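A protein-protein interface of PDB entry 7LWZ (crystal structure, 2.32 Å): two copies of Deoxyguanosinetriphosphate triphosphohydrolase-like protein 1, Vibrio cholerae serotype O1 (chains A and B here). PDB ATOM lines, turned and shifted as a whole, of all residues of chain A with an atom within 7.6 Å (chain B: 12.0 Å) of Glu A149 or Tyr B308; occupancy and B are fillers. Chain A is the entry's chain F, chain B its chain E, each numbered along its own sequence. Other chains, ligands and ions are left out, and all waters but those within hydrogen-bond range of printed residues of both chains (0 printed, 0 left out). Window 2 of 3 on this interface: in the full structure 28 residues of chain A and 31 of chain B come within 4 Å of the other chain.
Among the printed residues, pairs that only touch across the chains: Tyr A147 with Lys B311 (2.9 Å), Glu A149 with Tyr B308 (3.5 Å), Tyr A147 with Tyr B308 (3.5 Å), Pro A146 with Tyr B308 (3.6 Å) and Thr A148 with Tyr B308 (3.9 Å).
ND1 of His B307 lies within hydrogen-bond range of O of Pro A146 (3.1 Å).
The backbone carbonyl oxygen of Tyr B308 sits close to the side-chain amino group of Lys B311.
NZ of Lys B311 lies within salt-bridge range of OD2 of Asp B312 (3.8 Å).
The backbone NH of His A151 sits at hydrogen-bond distance from the side-chain hydroxyl of Thr A148.
The backbone carbonyl oxygen (O) of Gly A152 is in hydrogen-bond range of the side-chain hydroxyl (OG1) of Thr A148 (2.9 Å).
Pro A146 touches just these residues of chain B: His B307 (3.1 Å) and Tyr B308 (3.6 Å).
Thr A148 touches just one residue of chain B: Tyr B308.
Glu A149 touches one residue of chain B.
No residue of chain B comes within 4 Å of His A151.
Gly A152 touches none of the printed residues of chain B.
Of the printed residues of chain A, His B307 touches Pro A146.
Of the printed residues of chain A, Tyr B308 touches Pro A146, Tyr A147, Thr A148 and Glu A149.
Of the printed residues of chain A, Lys B311 touches Tyr A147.
The nearest printed residue of chain A that does not touch His B307 is Tyr A147 (4.4 Å).
No position is printed for both chains.
Of the 6 pairs that touch across the chains among the printed residues, none has its exchanged pair printed and touching as well.
Hydrophobic or aromatic side chains of chain A that line the printed part of chain B: Tyr A147.
Of the 23 printed residues of chain B, 3 touch a printed residue of chain A.
Printed residues of chain B that touch a printed residue of chain A: His B307, Tyr B308 and Lys B311.
Hydrophobic or aromatic side chains of chain B that line the printed part of chain A: His B307 and Tyr B308.
Along chain B the printed residues that touch a printed residue of chain A span positions 307 to 311.
Among the printed residues, 6 pairs touch across the chains.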
ATOM      1  N   ASN A  16       3.652  -0.825  28.786  1.00  0.00           N
ATOM      2  CA  ASN A  16       2.759  -0.192  27.778  1.00  0.00           C
ATOM      3  C   ASN A  16       1.351  -0.031  28.357  1.00  0.00           C
ATOM      4  O   ASN A  16       0.857  -0.991  28.973  1.00  0.00           O
ATOM      5  CB  ASN A  16       2.729  -0.989  26.471  1.00  0.00           C
ATOM      6  CG  ASN A  16       1.573  -0.612  25.571  1.00  0.00           C
ATOM      7  OD1 ASN A  16       0.413  -0.786  25.936  1.00  0.00           O
ATOM      8  ND2 ASN A  16       1.878  -0.091  24.393  1.00  0.00           N
ATOM      9  N   THR A 142       8.084 -10.805  29.721  1.00  0.00           N
ATOM     10  CA  THR A 142       8.250  -9.514  29.079  1.00  0.00           C
ATOM     11  C   THR A 142       8.057  -9.552  27.574  1.00  0.00           C
ATOM     12  O   THR A 142       7.870  -8.492  26.980  1.00  0.00           O
ATOM     13  CB  THR A 142       9.626  -8.921  29.411  1.00  0.00           C
ATOM     14  OG1 THR A 142      10.664  -9.755  28.887  1.00  0.00           O
ATOM     15  CG2 THR A 142       9.779  -8.799  30.941  1.00  0.00           C
ATOM     16  N   SER A 143       8.047 -10.729  26.942  1.00  0.00           N
ATOM     17  CA  SER A 143       7.974 -10.737  25.484  1.00  0.00           C
ATOM     18  C   SER A 143       7.202 -11.902  24.863  1.00  0.00           C
ATOM     19  O   SER A 143       6.379 -11.688  23.971  1.00  0.00           O
ATOM     20  CB  SER A 143       9.397 -10.726  24.931  1.00  0.00           C
ATOM     21  OG  SER A 143       9.369 -10.766  23.523  1.00  0.00           O
ATOM     22  N   GLU A 145       4.937 -14.454  26.026  1.00  0.00           N
ATOM     23  CA  GLU A 145       3.516 -14.765  26.219  1.00  0.00           C
ATOM     24  C   GLU A 145       2.706 -13.741  25.441  1.00  0.00           C
ATOM     25  O   GLU A 145       2.855 -12.544  25.673  1.00  0.00           O
ATOM     26  CB  GLU A 145       3.108 -14.775  27.692  1.00  0.00           C
ATOM     27  CG  GLU A 145       1.613 -15.098  27.900  1.00  0.00           C
ATOM     28  CD  GLU A 145       1.278 -16.599  27.758  1.00  0.00           C
ATOM     29  OE1 GLU A 145       0.157 -16.956  27.316  1.00  0.00           O
ATOM     30  OE2 GLU A 145       2.136 -17.434  28.095  1.00  0.00           O
ATOM     31  N   PRO A 146       1.892 -14.145  24.499  1.00  0.00           N
ATOM     32  CA  PRO A 146       1.291 -13.163  23.591  1.00  0.00           C
ATOM     33  C   PRO A 146       0.044 -12.522  24.166  1.00  0.00           C
ATOM     34  O   PRO A 146      -0.964 -12.395  23.466  1.00  0.00           O
ATOM     35  CB  PRO A 146       0.978 -13.987  22.333  1.00  0.00           C
ATOM     36  CG  PRO A 146       0.925 -15.392  22.771  1.00  0.00           C
ATOM     37  CD  PRO A 146       1.532 -15.525  24.151  1.00  0.00           C
ATOM     38  N   TYR A 147       0.093 -12.147  25.448  1.00  0.00           N
ATOM     39  CA  TYR A 147      -1.013 -11.417  26.067  1.00  0.00           C
ATOM     40  C   TYR A 147      -1.125 -10.006  25.508  1.00  0.00           C
ATOM     41  O   TYR A 147      -2.235  -9.480  25.373  1.00  0.00           O
ATOM     42  CB  TYR A 147      -0.848 -11.385  27.593  1.00  0.00           C
ATOM     43  CG  TYR A 147      -1.968 -10.671  28.334  1.00  0.00           C
ATOM     44  CD1 TYR A 147      -3.159 -11.324  28.640  1.00  0.00           C
ATOM     45  CD2 TYR A 147      -1.835  -9.345  28.730  1.00  0.00           C
ATOM     46  CE1 TYR A 147      -4.189 -10.673  29.327  1.00  0.00           C
ATOM     47  CE2 TYR A 147      -2.859  -8.684  29.400  1.00  0.00           C
ATOM     48  CZ  TYR A 147      -4.035  -9.353  29.698  1.00  0.00           C
ATOM     49  OH  TYR A 147      -5.055  -8.698  30.371  1.00  0.00           O
ATOM     50  N   THR A 148       0.011  -9.360  25.232  1.00  0.00           N
ATOM     51  CA  THR A 148       0.072  -8.119  24.461  1.00  0.00           C
ATOM     52  C   THR A 148       0.976  -8.332  23.256  1.00  0.00           C
ATOM     53  O   THR A 148       1.744  -9.295  23.193  1.00  0.00           O
ATOM     54  CB  THR A 148       0.595  -6.936  25.290  1.00  0.00           C
ATOM     55  OG1 THR A 148       1.980  -7.142  25.597  1.00  0.00           O
ATOM     56  CG2 THR A 148      -0.214  -6.754  26.585  1.00  0.00           C
ATOM     57  N   GLU A 149       0.928  -7.377  22.324  1.00  0.00           N
ATOM     58  CA  GLU A 149       1.623  -7.543  21.052  1.00  0.00           C
ATOM     59  C   GLU A 149       3.134  -7.421  21.194  1.00  0.00           C
ATOM     60  O   GLU A 149       3.879  -8.071  20.452  1.00  0.00           O
ATOM     61  CB  GLU A 149       1.104  -6.522  20.036  1.00  0.00           C
ATOM     62  CG  GLU A 149       1.682  -6.686  18.647  1.00  0.00           C
ATOM     63  CD  GLU A 149       1.125  -5.692  17.632  1.00  0.00           C
ATOM     64  OE1 GLU A 149       0.263  -4.861  17.995  1.00  0.00           O
ATOM     65  OE2 GLU A 149       1.551  -5.754  16.457  1.00  0.00           O
ATOM     66  N   HIS A 150       3.612  -6.581  22.110  1.00  0.00           N
ATOM     67  CA  HIS A 150       5.034  -6.298  22.188  1.00  0.00           C
ATOM     68  C   HIS A 150       5.618  -6.417  23.583  1.00  0.00           C
ATOM     69  O   HIS A 150       6.841  -6.337  23.728  1.00  0.00           O
ATOM     70  CB  HIS A 150       5.328  -4.889  21.652  1.00  0.00           C
ATOM     71  CG  HIS A 150       5.016  -4.723  20.200  1.00  0.00           C
ATOM     72  ND1 HIS A 150       4.240  -3.688  19.722  1.00  0.00           N
ATOM     73  CD2 HIS A 150       5.372  -5.461  19.122  1.00  0.00           C
ATOM     74  CE1 HIS A 150       4.136  -3.794  18.409  1.00  0.00           C
ATOM     75  NE2 HIS A 150       4.813  -4.860  18.020  1.00  0.00           N
ATOM     76  N   HIS A 151       4.802  -6.634  24.605  1.00  0.00           N
ATOM     77  CA  HIS A 151       5.331  -6.587  25.957  1.00  0.00           C
ATOM     78  C   HIS A 151       4.883  -7.789  26.781  1.00  0.00           C
ATOM     79  O   HIS A 151       4.755  -7.692  28.004  1.00  0.00           O
ATOM     80  CB  HIS A 151       4.941  -5.277  26.644  1.00  0.00           C
ATOM     81  CG  HIS A 151       5.441  -4.051  25.940  1.00  0.00           C
ATOM     82  ND1 HIS A 151       6.739  -3.599  26.055  1.00  0.00           N
ATOM     83  CD2 HIS A 151       4.811  -3.181  25.115  1.00  0.00           C
ATOM     84  CE1 HIS A 151       6.884  -2.501  25.335  1.00  0.00           C
ATOM     85  NE2 HIS A 151       5.730  -2.224  24.754  1.00  0.00           N
ATOM     86  N   GLY A 152       4.620  -8.916  26.128  1.00  0.00           N
ATOM     87  CA  GLY A 152       4.321 -10.136  26.863  1.00  0.00           C
ATOM     88  C   GLY A 152       3.101  -9.995  27.757  1.00  0.00           C
ATOM     89  O   GLY A 152       2.071  -9.444  27.353  1.00  0.00           O
ATOM     90  N   ASN A 154       2.936  -8.039  30.201  1.00  0.00           N
ATOM     91  CA  ASN A 154       2.868  -6.609  30.532  1.00  0.00           C
ATOM     92  C   ASN A 154       2.556  -6.389  32.008  1.00  0.00           C
ATOM     93  O   ASN A 154       1.609  -5.685  32.375  1.00  0.00           O
ATOM     94  CB  ASN A 154       1.847  -5.908  29.639  1.00  0.00           C
ATOM     95  CG  ASN A 154       1.920  -4.411  29.744  1.00  0.00           C
ATOM     96  OD1 ASN A 154       2.994  -3.855  29.941  1.00  0.00           O
ATOM     97  ND2 ASN A 154       0.774  -3.744  29.611  1.00  0.00           N
ATOM     98  N   LYS A 403       8.581 -16.214  12.705  1.00  0.00           N
ATOM     99  CA  LYS A 403       9.370 -15.456  13.670  1.00  0.00           C
ATOM    100  C   LYS A 403      10.862 -15.672  13.449  1.00  0.00           C
ATOM    101  O   LYS A 403      11.663 -14.770  13.721  1.00  0.00           O
ATOM    102  CB  LYS A 403       8.980 -15.817  15.100  1.00  0.00           C
ATOM    103  CG  LYS A 403       9.620 -14.873  16.131  1.00  0.00           C
ATOM    104  CD  LYS A 403       9.254 -15.179  17.588  1.00  0.00           C
ATOM    105  CE  LYS A 403       9.783 -14.089  18.523  1.00  0.00           C
ATOM    106  NZ  LYS A 403       8.751 -13.649  19.488  1.00  0.00           N
ATOM    107  N   ARG B  62      -5.390 -27.280  28.370  1.00  0.00           N
ATOM    108  CA  ARG B  62      -6.590 -26.878  29.141  1.00  0.00           C
ATOM    109  C   ARG B  62      -7.160 -28.139  29.789  1.00  0.00           C
ATOM    110  O   ARG B  62      -7.611 -29.034  29.063  1.00  0.00           O
ATOM    111  CB  ARG B  62      -7.590 -26.136  28.250  1.00  0.00           C
ATOM    112  CG  ARG B  62      -7.030 -24.854  27.652  1.00  0.00           C
ATOM    113  CD  ARG B  62      -8.030 -23.723  27.525  1.00  0.00           C
ATOM    114  NE  ARG B  62      -7.349 -22.473  27.233  1.00  0.00           N
ATOM    115  CZ  ARG B  62      -7.710 -21.290  27.707  1.00  0.00           C
ATOM    116  NH1 ARG B  62      -8.760 -21.188  28.502  1.00  0.00           N
ATOM    117  NH2 ARG B  62      -7.020 -20.212  27.385  1.00  0.00           N
ATOM    118  N   GLU B 262     -12.503 -20.383  22.831  1.00  0.00           N
ATOM    119  CA  GLU B 262     -11.381 -19.732  22.157  1.00  0.00           C
ATOM    120  C   GLU B 262     -10.467 -20.744  21.452  1.00  0.00           C
ATOM    121  O   GLU B 262     -10.095 -20.553  20.291  1.00  0.00           O
ATOM    122  CB  GLU B 262     -10.573 -18.888  23.133  1.00  0.00           C
ATOM    123  CG  GLU B 262      -9.572 -18.021  22.387  1.00  0.00           C
ATOM    124  CD  GLU B 262      -8.325 -17.712  23.185  1.00  0.00           C
ATOM    125  OE1 GLU B 262      -7.355 -17.199  22.576  1.00  0.00           O
ATOM    126  OE2 GLU B 262      -8.322 -17.967  24.412  1.00  0.00           O
ATOM    127  N   ILE B 265     -11.368 -22.259  18.159  1.00  0.00           N
ATOM    128  CA  ILE B 265     -11.157 -21.431  16.982  1.00  0.00           C
ATOM    129  C   ILE B 265      -9.746 -21.626  16.440  1.00  0.00           C
ATOM    130  O   ILE B 265      -9.534 -21.643  15.218  1.00  0.00           O
ATOM    131  CB  ILE B 265     -11.437 -19.951  17.308  1.00  0.00           C
ATOM    132  CG1 ILE B 265     -12.847 -19.758  17.887  1.00  0.00           C
ATOM    133  CG2 ILE B 265     -11.260 -19.122  16.081  1.00  0.00           C
ATOM    134  CD1 ILE B 265     -13.284 -18.303  17.902  1.00  0.00           C
ATOM    135  N   VAL B 266      -8.746 -21.745  17.328  1.00  0.00           N
ATOM    136  CA  VAL B 266      -7.369 -21.810  16.832  1.00  0.00           C
ATOM    137  C   VAL B 266      -7.038 -23.204  16.316  1.00  0.00           C
ATOM    138  O   VAL B 266      -6.293 -23.349  15.339  1.00  0.00           O
ATOM    139  CB  VAL B 266      -6.381 -21.359  17.920  1.00  0.00           C
ATOM    140  CG1 VAL B 266      -6.410 -22.305  19.104  1.00  0.00           C
ATOM    141  CG2 VAL B 266      -4.964 -21.266  17.339  1.00  0.00           C
ATOM    142  N   GLU B 297     -18.470  -6.924  15.909  1.00  0.00           N
ATOM    143  CA  GLU B 297     -17.087  -6.618  16.254  1.00  0.00           C
ATOM    144  C   GLU B 297     -16.429  -7.771  17.002  1.00  0.00           C
ATOM    145  O   GLU B 297     -15.237  -8.041  16.801  1.00  0.00           O
ATOM    146  CB  GLU B 297     -17.077  -5.338  17.089  1.00  0.00           C
ATOM    147  CG  GLU B 297     -15.744  -4.847  17.588  1.00  0.00           C
ATOM    148  CD  GLU B 297     -15.894  -3.532  18.352  1.00  0.00           C
ATOM    149  OE1 GLU B 297     -16.968  -2.902  18.237  1.00  0.00           O
ATOM    150  OE2 GLU B 297     -14.951  -3.127  19.063  1.00  0.00           O
ATOM    151  N   LEU B 298     -17.194  -8.485  17.830  1.00  0.00           N
ATOM    152  CA  LEU B 298     -16.659  -9.650  18.526  1.00  0.00           C
ATOM    153  C   LEU B 298     -16.296 -10.766  17.550  1.00  0.00           C
ATOM    154  O   LEU B 298     -15.309 -11.485  17.754  1.00  0.00           O
ATOM    155  CB  LEU B 298     -17.667 -10.147  19.562  1.00  0.00           C
ATOM    156  CG  LEU B 298     -17.888  -9.276  20.798  1.00  0.00           C
ATOM    157  CD1 LEU B 298     -19.194  -9.652  21.469  1.00  0.00           C
ATOM    158  CD2 LEU B 298     -16.724  -9.374  21.792  1.00  0.00           C
ATOM    159  N   GLU B 300     -15.260 -10.607  14.406  1.00  0.00           N
ATOM    160  CA  GLU B 300     -14.015 -10.366  13.627  1.00  0.00           C
ATOM    161  C   GLU B 300     -12.801 -10.457  14.550  1.00  0.00           C
ATOM    162  O   GLU B 300     -11.727 -10.836  14.075  1.00  0.00           O
ATOM    163  CB  GLU B 300     -14.062  -9.001  12.937  1.00  0.00           C
ATOM    164  N   MET B 301     -12.964 -10.088  15.816  1.00  0.00           N
ATOM    165  CA  MET B 301     -11.860 -10.207  16.768  1.00  0.00           C
ATOM    166  C   MET B 301     -11.544 -11.663  17.107  1.00  0.00           C
ATOM    167  O   MET B 301     -10.375 -12.020  17.317  1.00  0.00           O
ATOM    168  CB  MET B 301     -12.190  -9.474  18.067  1.00  0.00           C
ATOM    169  CG  MET B 301     -12.218  -7.946  18.057  1.00  0.00           C
ATOM    170  SD  MET B 301     -12.868  -7.284  19.615  1.00  0.00           S
ATOM    171  CE  MET B 301     -11.401  -6.630  20.419  1.00  0.00           C
ATOM    172  N   LEU B 302     -12.572 -12.510  17.193  1.00  0.00           N
ATOM    173  CA  LEU B 302     -12.359 -13.916  17.525  1.00  0.00           C
ATOM    174  C   LEU B 302     -11.634 -14.645  16.403  1.00  0.00           C
ATOM    175  O   LEU B 302     -10.897 -15.608  16.654  1.00  0.00           O
ATOM    176  CB  LEU B 302     -13.696 -14.590  17.848  1.00  0.00           C
ATOM    177  CG  LEU B 302     -14.362 -14.148  19.167  1.00  0.00           C
ATOM    178  CD1 LEU B 302     -15.740 -14.797  19.381  1.00  0.00           C
ATOM    179  CD2 LEU B 302     -13.440 -14.430  20.352  1.00  0.00           C
ATOM    180  N   PHE B 303     -11.814 -14.193  15.167  1.00  0.00           N
ATOM    181  CA  PHE B 303     -11.143 -14.790  14.024  1.00  0.00           C
ATOM    182  C   PHE B 303     -10.001 -13.924  13.517  1.00  0.00           C
ATOM    183  O   PHE B 303      -9.562 -14.093  12.371  1.00  0.00           O
ATOM    184  CB  PHE B 303     -12.163 -15.102  12.927  1.00  0.00           C
ATOM    185  CG  PHE B 303     -13.112 -16.200  13.331  1.00  0.00           C
ATOM    186  CD1 PHE B 303     -14.266 -15.909  14.052  1.00  0.00           C
ATOM    187  CD2 PHE B 303     -12.802 -17.531  13.088  1.00  0.00           C
ATOM    188  CE1 PHE B 303     -15.122 -16.920  14.474  1.00  0.00           C
ATOM    189  CE2 PHE B 303     -13.652 -18.546  13.508  1.00  0.00           C
ATOM    190  CZ  PHE B 303     -14.812 -18.236  14.205  1.00  0.00           C
ATOM    191  N   SER B 304      -9.488 -13.039  14.380  1.00  0.00           N
ATOM    192  CA  SER B 304      -8.292 -12.252  14.096  1.00  0.00           C
ATOM    193  C   SER B 304      -7.070 -13.093  13.743  1.00  0.00           C
ATOM    194  O   SER B 304      -6.209 -12.637  12.984  1.00  0.00           O
ATOM    195  CB  SER B 304      -7.967 -11.401  15.313  1.00  0.00           C
ATOM    196  OG  SER B 304      -6.566 -11.233  15.404  1.00  0.00           O
ATOM    197  N   GLY B 305      -6.920 -14.268  14.354  1.00  0.00           N
ATOM    198  CA  GLY B 305      -5.675 -15.020  14.258  1.00  0.00           C
ATOM    199  C   GLY B 305      -4.557 -14.495  15.125  1.00  0.00           C
ATOM    200  O   GLY B 305      -3.446 -15.022  15.048  1.00  0.00           O
ATOM    201  N   LYS B 306      -4.833 -13.503  15.971  1.00  0.00           N
ATOM    202  CA  LYS B 306      -3.861 -12.910  16.880  1.00  0.00           C
ATOM    203  C   LYS B 306      -4.419 -13.034  18.290  1.00  0.00           C
ATOM    204  O   LYS B 306      -5.558 -12.635  18.544  1.00  0.00           O
ATOM    205  CB  LYS B 306      -3.591 -11.444  16.529  1.00  0.00           C
ATOM    206  CG  LYS B 306      -2.985 -11.198  15.150  1.00  0.00           C
ATOM    207  CD  LYS B 306      -1.487 -11.468  15.147  1.00  0.00           C
ATOM    208  CE  LYS B 306      -1.168 -12.810  14.513  1.00  0.00           C
ATOM    209  NZ  LYS B 306       0.086 -13.384  15.061  1.00  0.00           N
ATOM    210  N   HIS B 307      -3.631 -13.620  19.192  1.00  0.00           N
ATOM    211  CA  HIS B 307      -4.117 -13.890  20.543  1.00  0.00           C
ATOM    212  C   HIS B 307      -4.419 -12.605  21.312  1.00  0.00           C
ATOM    213  O   HIS B 307      -5.397 -12.537  22.066  1.00  0.00           O
ATOM    214  CB  HIS B 307      -3.107 -14.737  21.306  1.00  0.00           C
ATOM    215  CG  HIS B 307      -3.586 -15.158  22.654  1.00  0.00           C
ATOM    216  ND1 HIS B 307      -3.155 -14.559  23.820  1.00  0.00           N
ATOM    217  CD2 HIS B 307      -4.483 -16.104  23.024  1.00  0.00           C
ATOM    218  CE1 HIS B 307      -3.756 -15.129  24.849  1.00  0.00           C
ATOM    219  NE2 HIS B 307      -4.568 -16.067  24.395  1.00  0.00           N
ATOM    220  N   TYR B 308      -3.581 -11.581  21.156  1.00  0.00           N
ATOM    221  CA  TYR B 308      -3.752 -10.396  21.982  1.00  0.00           C
ATOM    222  C   TYR B 308      -5.020  -9.609  21.662  1.00  0.00           C
ATOM    223  O   TYR B 308      -5.435  -8.788  22.484  1.00  0.00           O
ATOM    224  CB  TYR B 308      -2.525  -9.489  21.851  1.00  0.00           C
ATOM    225  CG  TYR B 308      -2.106  -9.176  20.435  1.00  0.00           C
ATOM    226  CD1 TYR B 308      -2.811  -8.255  19.661  1.00  0.00           C
ATOM    227  CD2 TYR B 308      -0.983  -9.776  19.877  1.00  0.00           C
ATOM    228  CE1 TYR B 308      -2.419  -7.956  18.361  1.00  0.00           C
ATOM    229  CE2 TYR B 308      -0.579  -9.481  18.573  1.00  0.00           C
ATOM    230  CZ  TYR B 308      -1.301  -8.575  17.822  1.00  0.00           C
ATOM    231  OH  TYR B 308      -0.902  -8.288  16.535  1.00  0.00           O
ATOM    232  N   VAL B 309      -5.649  -9.829  20.512  1.00  0.00           N
ATOM    233  CA  VAL B 309      -6.954  -9.244  20.221  1.00  0.00           C
ATOM    234  C   VAL B 309      -8.087 -10.226  20.517  1.00  0.00           C
ATOM    235  O   VAL B 309      -9.178  -9.816  20.916  1.00  0.00           O
ATOM    236  CB  VAL B 309      -7.006  -8.692  18.777  1.00  0.00           C
ATOM    237  CG1 VAL B 309      -6.458  -9.677  17.823  1.00  0.00           C
ATOM    238  CG2 VAL B 309      -8.415  -8.273  18.390  1.00  0.00           C
ATOM    239  N   ARG B 310      -7.864 -11.526  20.298  1.00  0.00           N
ATOM    240  CA  ARG B 310      -8.879 -12.508  20.669  1.00  0.00           C
ATOM    241  C   ARG B 310      -9.199 -12.448  22.159  1.00  0.00           C
ATOM    242  O   ARG B 310     -10.358 -12.598  22.561  1.00  0.00           O
ATOM    243  CB  ARG B 310      -8.393 -13.921  20.349  1.00  0.00           C
ATOM    244  CG  ARG B 310      -8.490 -14.403  18.942  1.00  0.00           C
ATOM    245  CD  ARG B 310      -8.509 -15.934  18.969  1.00  0.00           C
ATOM    246  NE  ARG B 310      -7.230 -16.504  19.395  1.00  0.00           N
ATOM    247  CZ  ARG B 310      -6.233 -16.790  18.562  1.00  0.00           C
ATOM    248  NH1 ARG B 310      -6.365 -16.559  17.264  1.00  0.00           N
ATOM    249  NH2 ARG B 310      -5.111 -17.311  19.027  1.00  0.00           N
ATOM    250  N   LYS B 311      -8.166 -12.292  22.994  1.00  0.00           N
ATOM    251  CA  LYS B 311      -8.366 -12.162  24.437  1.00  0.00           C
ATOM    252  C   LYS B 311      -9.289 -10.997  24.781  1.00  0.00           C
ATOM    253  O   LYS B 311     -10.053 -11.084  25.755  1.00  0.00           O
ATOM    254  CB  LYS B 311      -7.020 -12.029  25.156  1.00  0.00           C
ATOM    255  CG  LYS B 311      -6.277 -10.717  24.897  1.00  0.00           C
ATOM    256  CD  LYS B 311      -5.856 -10.092  26.219  1.00  0.00           C
ATOM    257  CE  LYS B 311      -4.977  -8.870  26.047  1.00  0.00           C
ATOM    258  NZ  LYS B 311      -5.734  -7.697  25.573  1.00  0.00           N
ATOM    259  N   ASP B 312      -9.235  -9.905  24.002  1.00  0.00           N
ATOM    260  CA  ASP B 312     -10.085  -8.753  24.282  1.00  0.00           C
ATOM    261  C   ASP B 312     -11.551  -9.101  24.095  1.00  0.00           C
ATOM    262  O   ASP B 312     -12.412  -8.632  24.851  1.00  0.00           O
ATOM    263  CB  ASP B 312      -9.727  -7.580  23.366  1.00  0.00           C
ATOM    264  CG  ASP B 312      -8.370  -6.976  23.669  1.00  0.00           C
ATOM    265  OD1 ASP B 312      -7.869  -7.162  24.795  1.00  0.00           O
ATOM    266  OD2 ASP B 312      -7.810  -6.302  22.775  1.00  0.00           O
ATOM    267  N   ALA B 313     -11.855  -9.921  23.092  1.00  0.00           N
ATOM    268  CA  ALA B 313     -13.230 -10.355  22.890  1.00  0.00           C
ATOM    269  C   ALA B 313     -13.683 -11.259  24.025  1.00  0.00           C
ATOM    270  O   ALA B 313     -14.737 -11.024  24.634  1.00  0.00           O
ATOM    271  CB  ALA B 313     -13.361 -11.060  21.536  1.00  0.00           C
ATOM    272  N   ILE B 314     -12.864 -12.269  24.356  1.00  0.00           N
ATOM    273  CA  ILE B 314     -13.194 -13.196  25.439  1.00  0.00           C
ATOM    274  C   ILE B 314     -13.401 -12.426  26.735  1.00  0.00           C
ATOM    275  O   ILE B 314     -14.351 -12.678  27.487  1.00  0.00           O
ATOM    276  CB  ILE B 314     -12.089 -14.263  25.589  1.00  0.00           C
ATOM    277  CG1 ILE B 314     -11.879 -15.046  24.284  1.00  0.00           C
ATOM    278  CG2 ILE B 314     -12.400 -15.225  26.751  1.00  0.00           C
ATOM    279  CD1 ILE B 314     -12.992 -15.992  23.944  1.00  0.00           C
ATOM    280  N   GLY B 315     -12.505 -11.475  27.018  1.00  0.00           N
ATOM    281  CA  GLY B 315     -12.655 -10.664  28.214  1.00  0.00           C
ATOM    282  C   GLY B 315     -13.922  -9.834  28.189  1.00  0.00           C
ATOM    283  O   GLY B 315     -14.622  -9.724  29.195  1.00  0.00           O
ATOM    284  N   GLY B 316     -14.255  -9.268  27.028  1.00  0.00           N
ATOM    285  CA  GLY B 316     -15.469  -8.476  26.928  1.00  0.00           C
ATOM    286  C   GLY B 316     -16.723  -9.311  27.113  1.00  0.00           C
ATOM    287  O   GLY B 316     -17.730  -8.824  27.629  1.00  0.00           O
